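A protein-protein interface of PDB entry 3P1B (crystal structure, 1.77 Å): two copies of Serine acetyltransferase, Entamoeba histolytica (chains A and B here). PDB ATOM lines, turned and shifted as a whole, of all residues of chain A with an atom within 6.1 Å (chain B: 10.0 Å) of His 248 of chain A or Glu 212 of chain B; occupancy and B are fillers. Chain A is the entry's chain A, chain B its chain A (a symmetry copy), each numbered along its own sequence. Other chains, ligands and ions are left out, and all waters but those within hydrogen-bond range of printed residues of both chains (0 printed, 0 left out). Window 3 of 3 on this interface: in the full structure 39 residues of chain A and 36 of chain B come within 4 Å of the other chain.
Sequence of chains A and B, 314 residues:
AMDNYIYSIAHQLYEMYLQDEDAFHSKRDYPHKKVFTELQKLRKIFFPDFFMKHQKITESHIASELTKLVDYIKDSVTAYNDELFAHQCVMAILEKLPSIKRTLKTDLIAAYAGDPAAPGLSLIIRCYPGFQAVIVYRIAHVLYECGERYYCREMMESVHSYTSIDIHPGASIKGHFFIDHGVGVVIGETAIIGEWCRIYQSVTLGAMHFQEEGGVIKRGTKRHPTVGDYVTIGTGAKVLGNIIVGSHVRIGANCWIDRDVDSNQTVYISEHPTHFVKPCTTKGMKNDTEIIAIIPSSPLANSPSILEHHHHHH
Arg 198 of chain A touches Gln 211 of chain B.
NE2 of Gln 211 of chain B touches CD1 of Tyr 230 of chain A, at 3.7 Å.
CD1 of Tyr 230 of chain A touches OE1 of Glu 212 of chain B (3.5 Å).
His 248 of chain A touches Glu 212 of chain B (CD2 to OE1, 3.9 Å).
Arg 250 of chain A touches Phe 210 of chain B (NH1 to CB, 3.4 Å).
Thr 266 of chain A touches Phe 210 of chain B.
N of Arg 198 of chain A is in hydrogen-bond range of O of Val 231 of chain A, 3.1 Å away.
The backbone carbonyl oxygen (O) of Asp 229 of chain A lies within hydrogen-bond range of the backbone NH (N) of His 248 of chain A (3.0 Å).
The backbone carbonyl oxygen of His 248 of chain A sits close to the backbone NH of Asn 264 of chain A, at 3.3 Å.
O of His 248 of chain A lies within hydrogen-bond range of N of Gln 265 of chain A (3.4 Å).
The backbone NH of Arg 250 of chain A sits at hydrogen-bond distance from the backbone carbonyl oxygen of Gln 265 of chain A (3.1 Å).
No position is printed for both chains.
Of the 9 pairs that touch across the chains among the printed residues, none has its exchanged pair printed and touching as well.
Glu 212 of chain B touches just these residues of chain A: Tyr 230 (3.5 Å) and His 248 (3.9 Å).
No residue of chain B comes within 4 Å of Ser 247 of chain A.
No residue of chain B comes within 4 Å of Val 249 of chain A.
No residue of chain B comes within 4 Å of Asn 264 of chain A.
Of the printed residues of chain B, Val 231 of chain A touches Gln 211.
Of the printed residues of chain A, Phe 210 of chain B touches Arg 250 and Thr 266.
Of the printed residues of chain B, Arg 250 of chain A touches Phe 210 (3.4 Å) and Gln 211 (3.1 Å).
Gly 246 of chain A touches none of the printed residues of chain B.
The nearest residue of chain B that does not touch His 248 of chain A is Gln 211 of chain B (6.6 Å).
The nearest residue of chain A that does not touch Glu 212 of chain B is Arg 250 of chain A (4.1 Å).
The nearest printed residue of chain B that does not touch Arg 250 of chain A is Glu 212 of chain B (4.1 Å).
The guanidinium group (NH1) of Arg 198 of chain A is in hydrogen-bond range of the backbone carbonyl oxygen (O) of His 209 of chain B (3.0 Å).
The backbone carbonyl oxygen of Val 231 of chain A lies close to the side-chain amide oxygen of Gln 211 of chain B, 3.4 Å away.
NH2 of Arg 250 of chain A is in hydrogen-bond range of O of Gln 211 of chain B (3.1 Å).
Hydrophobic or aromatic side chains of chain B within 4 Å of the printed part of chain A: His 209 and Phe 210.
Among the printed residues, no Asp or Glu carboxylate lies within 4 Å of a Lys or Arg side-chain nitrogen of the other chain.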
ATOM      1  N   ARG A 198      27.856 -15.785  -9.074  1.00  0.00           N
ATOM      2  CA  ARG A 198      27.241 -14.882  -8.088  1.00  0.00           C
ATOM      3  C   ARG A 198      28.173 -14.868  -6.887  1.00  0.00           C
ATOM      4  O   ARG A 198      28.486 -15.899  -6.319  1.00  0.00           O
ATOM      5  CB  ARG A 198      25.883 -15.446  -7.641  1.00  0.00           C
ATOM      6  CG  ARG A 198      25.196 -14.674  -6.533  1.00  0.00           C
ATOM      7  CD  ARG A 198      23.818 -15.331  -6.212  1.00  0.00           C
ATOM      8  NE  ARG A 198      23.066 -15.549  -7.451  1.00  0.00           N
ATOM      9  CZ  ARG A 198      21.874 -16.137  -7.572  1.00  0.00           C
ATOM     10  NH1 ARG A 198      21.240 -16.616  -6.524  1.00  0.00           N
ATOM     11  NH2 ARG A 198      21.297 -16.231  -8.762  1.00  0.00           N
ATOM     12  N   GLY A 228      34.142 -22.322 -12.742  1.00  0.00           N
ATOM     13  CA  GLY A 228      33.228 -22.688 -13.836  1.00  0.00           C
ATOM     14  C   GLY A 228      31.941 -21.857 -13.905  1.00  0.00           C
ATOM     15  O   GLY A 228      31.903 -20.717 -13.418  1.00  0.00           O
ATOM     16  N   ASP A 229      30.875 -22.449 -14.458  1.00  0.00           N
ATOM     17  CA  ASP A 229      29.622 -21.744 -14.717  1.00  0.00           C
ATOM     18  C   ASP A 229      28.648 -22.027 -13.563  1.00  0.00           C
ATOM     19  O   ASP A 229      28.770 -23.045 -12.943  1.00  0.00           O
ATOM     20  CB  ASP A 229      29.023 -22.279 -16.017  1.00  0.00           C
ATOM     21  CG  ASP A 229      29.810 -21.851 -17.287  1.00  0.00           C
ATOM     22  OD1 ASP A 229      30.512 -20.788 -17.336  1.00  0.00           O
ATOM     23  OD2 ASP A 229      29.656 -22.595 -18.288  1.00  0.00           O
ATOM     24  N   TYR A 230      27.677 -21.148 -13.272  1.00  0.00           N
ATOM     25  CA  TYR A 230      26.712 -21.420 -12.170  1.00  0.00           C
ATOM     26  C   TYR A 230      27.358 -21.666 -10.793  1.00  0.00           C
ATOM     27  O   TYR A 230      26.934 -22.534 -10.028  1.00  0.00           O
ATOM     28  CB  TYR A 230      25.736 -22.579 -12.543  1.00  0.00           C
ATOM     29  CG  TYR A 230      25.043 -22.299 -13.846  1.00  0.00           C
ATOM     30  CD1 TYR A 230      23.873 -21.533 -13.890  1.00  0.00           C
ATOM     31  CD2 TYR A 230      25.583 -22.754 -15.052  1.00  0.00           C
ATOM     32  CE1 TYR A 230      23.263 -21.235 -15.106  1.00  0.00           C
ATOM     33  CE2 TYR A 230      24.980 -22.455 -16.277  1.00  0.00           C
ATOM     34  CZ  TYR A 230      23.823 -21.697 -16.291  1.00  0.00           C
ATOM     35  OH  TYR A 230      23.211 -21.395 -17.485  1.00  0.00           O
ATOM     36  N   VAL A 231      28.393 -20.908 -10.464  1.00  0.00           N
ATOM     37  CA  VAL A 231      29.060 -21.050  -9.171  1.00  0.00           C
ATOM     38  C   VAL A 231      28.598 -19.954  -8.179  1.00  0.00           C
ATOM     39  O   VAL A 231      28.563 -18.805  -8.539  1.00  0.00           O
ATOM     40  CB  VAL A 231      30.615 -21.000  -9.326  1.00  0.00           C
ATOM     41  CG1 VAL A 231      31.302 -20.963  -8.009  1.00  0.00           C
ATOM     42  CG2 VAL A 231      31.136 -22.216 -10.109  1.00  0.00           C
ATOM     43  N   GLY A 246      34.833 -26.388 -10.201  1.00  0.00           N
ATOM     44  CA  GLY A 246      33.983 -26.806 -11.318  1.00  0.00           C
ATOM     45  C   GLY A 246      32.687 -26.026 -11.361  1.00  0.00           C
ATOM     46  O   GLY A 246      32.470 -25.132 -10.529  1.00  0.00           O
ATOM     47  N   SER A 247      31.821 -26.376 -12.319  1.00  0.00           N
ATOM     48  CA  SER A 247      30.513 -25.759 -12.475  1.00  0.00           C
ATOM     49  C   SER A 247      29.506 -26.279 -11.449  1.00  0.00           C
ATOM     50  O   SER A 247      29.695 -27.369 -10.872  1.00  0.00           O
ATOM     51  CB  SER A 247      29.998 -25.958 -13.903  1.00  0.00           C
ATOM     52  OG  SER A 247      30.947 -25.500 -14.859  1.00  0.00           O
ATOM     53  N   HIS A 248      28.454 -25.493 -11.200  1.00  0.00           N
ATOM     54  CA  HIS A 248      27.411 -25.830 -10.217  1.00  0.00           C
ATOM     55  C   HIS A 248      27.991 -26.163  -8.839  1.00  0.00           C
ATOM     56  O   HIS A 248      27.641 -27.190  -8.272  1.00  0.00           O
ATOM     57  CB  HIS A 248      26.528 -27.002 -10.729  1.00  0.00           C
ATOM     58  CG  HIS A 248      25.865 -26.709 -12.048  1.00  0.00           C
ATOM     59  ND1 HIS A 248      26.436 -27.054 -13.256  1.00  0.00           N
ATOM     60  CD2 HIS A 248      24.724 -26.037 -12.350  1.00  0.00           C
ATOM     61  CE1 HIS A 248      25.666 -26.632 -14.248  1.00  0.00           C
ATOM     62  NE2 HIS A 248      24.620 -26.015 -13.723  1.00  0.00           N
ATOM     63  N   VAL A 249      28.936 -25.345  -8.365  1.00  0.00           N
ATOM     64  CA  VAL A 249      29.498 -25.461  -7.028  1.00  0.00           C
ATOM     65  C   VAL A 249      28.896 -24.309  -6.211  1.00  0.00           C
ATOM     66  O   VAL A 249      28.736 -23.211  -6.711  1.00  0.00           O
ATOM     67  CB  VAL A 249      31.051 -25.401  -7.088  1.00  0.00           C
ATOM     68  CG1 VAL A 249      31.685 -25.329  -5.701  1.00  0.00           C
ATOM     69  CG2 VAL A 249      31.570 -26.639  -7.852  1.00  0.00           C
ATOM     70  N   ARG A 250      28.487 -24.593  -4.985  1.00  0.00           N
ATOM     71  CA  ARG A 250      28.082 -23.526  -4.060  1.00  0.00           C
ATOM     72  C   ARG A 250      29.054 -23.642  -2.917  1.00  0.00           C
ATOM     73  O   ARG A 250      29.248 -24.714  -2.378  1.00  0.00           O
ATOM     74  CB  ARG A 250      26.670 -23.744  -3.564  1.00  0.00           C
ATOM     75  CG  ARG A 250      25.647 -23.949  -4.663  1.00  0.00           C
ATOM     76  CD  ARG A 250      24.770 -25.171  -4.292  1.00  0.00           C
ATOM     77  NE  ARG A 250      23.688 -25.419  -5.243  1.00  0.00           N
ATOM     78  CZ  ARG A 250      22.388 -25.479  -4.931  1.00  0.00           C
ATOM     79  NH1 ARG A 250      21.974 -25.326  -3.670  1.00  0.00           N
ATOM     80  NH2 ARG A 250      21.495 -25.703  -5.896  1.00  0.00           N
ATOM     81  N   ASP A 262      35.410 -30.232  -7.309  1.00  0.00           N
ATOM     82  CA  ASP A 262      34.706 -30.917  -8.388  1.00  0.00           C
ATOM     83  C   ASP A 262      33.348 -30.279  -8.647  1.00  0.00           C
ATOM     84  O   ASP A 262      32.703 -29.790  -7.711  1.00  0.00           O
ATOM     85  CB  ASP A 262      34.510 -32.392  -8.029  1.00  0.00           C
ATOM     86  CG  ASP A 262      35.813 -33.188  -8.070  1.00  0.00           C
ATOM     87  OD1 ASP A 262      36.754 -32.770  -8.796  1.00  0.00           O
ATOM     88  OD2 ASP A 262      35.905 -34.222  -7.366  1.00  0.00           O
ATOM     89  N   SER A 263      32.921 -30.292  -9.910  1.00  0.00           N
ATOM     90  CA  SER A 263      31.587 -29.825 -10.295  1.00  0.00           C
ATOM     91  C   SER A 263      30.452 -30.462  -9.467  1.00  0.00           C
ATOM     92  O   SER A 263      30.624 -31.521  -8.836  1.00  0.00           O
ATOM     93  CB  SER A 263      31.343 -30.065 -11.783  1.00  0.00           C
ATOM     94  OG  SER A 263      32.076 -29.161 -12.597  1.00  0.00           O
ATOM     95  N   ASN A 264      29.306 -29.784  -9.444  1.00  0.00           N
ATOM     96  CA  ASN A 264      28.069 -30.308  -8.841  1.00  0.00           C
ATOM     97  C   ASN A 264      28.109 -30.606  -7.326  1.00  0.00           C
ATOM     98  O   ASN A 264      27.430 -31.532  -6.852  1.00  0.00           O
ATOM     99  CB  ASN A 264      27.576 -31.538  -9.630  1.00  0.00           C
ATOM    100  CG  ASN A 264      27.470 -31.271 -11.129  1.00  0.00           C
ATOM    101  OD1 ASN A 264      26.524 -30.636 -11.597  1.00  0.00           O
ATOM    102  ND2 ASN A 264      28.431 -31.790 -11.891  1.00  0.00           N
ATOM    103  N   GLN A 265      28.881 -29.814  -6.574  1.00  0.00           N
ATOM    104  CA  GLN A 265      29.011 -29.978  -5.120  1.00  0.00           C
ATOM    105  C   GLN A 265      28.479 -28.785  -4.316  1.00  0.00           C
ATOM    106  O   GLN A 265      28.342 -27.681  -4.835  1.00  0.00           O
ATOM    107  CB  GLN A 265      30.484 -30.131  -4.738  1.00  0.00           C
ATOM    108  CG  GLN A 265      31.111 -31.508  -4.919  1.00  0.00           C
ATOM    109  CD  GLN A 265      32.408 -31.643  -4.114  1.00  0.00           C
ATOM    110  OE1 GLN A 265      33.522 -31.496  -4.643  1.00  0.00           O
ATOM    111  NE2 GLN A 265      32.260 -31.915  -2.818  1.00  0.00           N
ATOM    112  N   THR A 266      28.209 -29.026  -3.032  1.00  0.00           N
ATOM    113  CA  THR A 266      28.084 -27.963  -2.048  1.00  0.00           C
ATOM    114  C   THR A 266      29.183 -28.111  -0.996  1.00  0.00           C
ATOM    115  O   THR A 266      29.359 -29.173  -0.409  1.00  0.00           O
ATOM    116  CB  THR A 266      26.683 -27.914  -1.412  1.00  0.00           C
ATOM    117  OG1 THR A 266      25.712 -27.718  -2.446  1.00  0.00           O
ATOM    118  CG2 THR A 266      26.571 -26.750  -0.428  1.00  0.00           C
ATOM    119  N   HIS B 209      22.178 -16.765  -1.326  1.00  0.00           N
ATOM    120  CA  HIS B 209      21.258 -17.539  -2.170  1.00  0.00           C
ATOM    121  C   HIS B 209      22.002 -18.407  -3.190  1.00  0.00           C
ATOM    122  O   HIS B 209      22.544 -17.906  -4.187  1.00  0.00           O
ATOM    123  CB  HIS B 209      20.252 -16.605  -2.859  1.00  0.00           C
ATOM    124  CG  HIS B 209      19.531 -15.698  -1.909  1.00  0.00           C
ATOM    125  ND1 HIS B 209      18.560 -16.150  -1.039  1.00  0.00           N
ATOM    126  CD2 HIS B 209      19.649 -14.366  -1.686  1.00  0.00           C
ATOM    127  CE1 HIS B 209      18.106 -15.135  -0.324  1.00  0.00           C
ATOM    128  NE2 HIS B 209      18.753 -14.042  -0.691  1.00  0.00           N
ATOM    129  N   PHE B 210      22.081 -19.700  -2.913  1.00  0.00           N
ATOM    130  CA  PHE B 210      22.664 -20.625  -3.897  1.00  0.00           C
ATOM    131  C   PHE B 210      21.776 -20.688  -5.137  1.00  0.00           C
ATOM    132  O   PHE B 210      20.549 -20.642  -5.030  1.00  0.00           O
ATOM    133  CB  PHE B 210      22.873 -22.023  -3.311  1.00  0.00           C
ATOM    134  CG  PHE B 210      23.906 -22.072  -2.237  1.00  0.00           C
ATOM    135  CD1 PHE B 210      23.912 -23.112  -1.307  1.00  0.00           C
ATOM    136  CD2 PHE B 210      24.878 -21.075  -2.142  1.00  0.00           C
ATOM    137  CE1 PHE B 210      24.861 -23.169  -0.306  1.00  0.00           C
ATOM    138  CE2 PHE B 210      25.831 -21.113  -1.143  1.00  0.00           C
ATOM    139  CZ  PHE B 210      25.822 -22.171  -0.214  1.00  0.00           C
ATOM    140  N   GLN B 211      22.396 -20.816  -6.305  1.00  0.00           N
ATOM    141  CA  GLN B 211      21.666 -20.806  -7.583  1.00  0.00           C
ATOM    142  C   GLN B 211      20.782 -22.038  -7.830  1.00  0.00           C
ATOM    143  O   GLN B 211      21.213 -23.187  -7.604  1.00  0.00           O
ATOM    144  CB  GLN B 211      22.642 -20.615  -8.759  1.00  0.00           C
ATOM    145  CG  GLN B 211      22.977 -19.157  -9.016  1.00  0.00           C
ATOM    146  CD  GLN B 211      24.125 -18.946 -10.000  1.00  0.00           C
ATOM    147  OE1 GLN B 211      25.289 -18.776  -9.602  1.00  0.00           O
ATOM    148  NE2 GLN B 211      23.797 -18.934 -11.291  1.00  0.00           N
ATOM    149  N   GLU B 212      19.563 -21.773  -8.320  1.00  0.00           N
ATOM    150  CA  GLU B 212      18.602 -22.799  -8.778  1.00  0.00           C
ATOM    151  C   GLU B 212      18.361 -23.843  -7.679  1.00  0.00           C
ATOM    152  O   GLU B 212      17.263 -23.948  -7.119  1.00  0.00           O
ATOM    153  CB  GLU B 212      19.079 -23.528 -10.056  1.00  0.00           C
ATOM    154  CG  GLU B 212      19.971 -22.740 -11.060  1.00  0.00           C
ATOM    155  CD  GLU B 212      21.299 -23.469 -11.367  1.00  0.00           C
ATOM    156  OE1 GLU B 212      21.580 -23.762 -12.558  1.00  0.00           O
ATOM    157  OE2 GLU B 212      22.056 -23.770 -10.406  1.00  0.00           O
ATOM    158  N   VAL B 216      15.011 -16.782 -11.194  1.00  0.00           N
ATOM    159  CA  VAL B 216      14.534 -15.511 -10.612  1.00  0.00           C
ATOM    160  C   VAL B 216      13.980 -15.753  -9.201  1.00  0.00           C
ATOM    161  O   VAL B 216      12.830 -16.185  -9.009  1.00  0.00           O
ATOM    162  CB  VAL B 216      13.501 -14.781 -11.489  1.00  0.00           C
ATOM    163  CG1 VAL B 216      13.422 -13.320 -11.090  1.00  0.00           C
ATOM    164  CG2 VAL B 216      13.860 -14.876 -12.967  1.00  0.00           C
ATOM    165  N   ILE B 217      14.806 -15.469  -8.229  1.00  0.00           N
ATOM    166  CA  ILE B 217      14.509 -15.801  -6.870  1.00  0.00           C
ATOM    167  C   ILE B 217      13.337 -15.016  -6.359  1.00  0.00           C
ATOM    168  O   ILE B 217      13.074 -13.966  -6.831  1.00  0.00           O
ATOM    169  CB  ILE B 217      15.709 -15.647  -6.026  1.00  0.00           C
ATOM    170  CG1 ILE B 217      15.524 -16.370  -4.735  1.00  0.00           C
ATOM    171  CG2 ILE B 217      15.974 -14.261  -5.777  1.00  0.00           C
ATOM    172  CD1 ILE B 217      16.716 -16.317  -3.887  1.00  0.00           C
ATOM    173  N   LYS B 218      12.586 -15.573  -5.429  1.00  0.00           N
ATOM    174  CA  LYS B 218      11.397 -14.869  -4.976  1.00  0.00           C
ATOM    175  C   LYS B 218      11.743 -13.539  -4.369  1.00  0.00           C
ATOM    176  O   LYS B 218      12.777 -13.397  -3.799  1.00  0.00           O
ATOM    177  CB  LYS B 218      10.593 -15.701  -4.007  1.00  0.00           C
ATOM    178  CG  LYS B 218      11.338 -16.314  -2.950  1.00  0.00           C
ATOM    179  CD  LYS B 218      10.333 -16.620  -1.878  1.00  0.00           C
ATOM    180  CE  LYS B 218      10.961 -17.138  -0.692  1.00  0.00           C
ATOM    181  NZ  LYS B 218      11.534 -18.456  -0.966  1.00  0.00           N
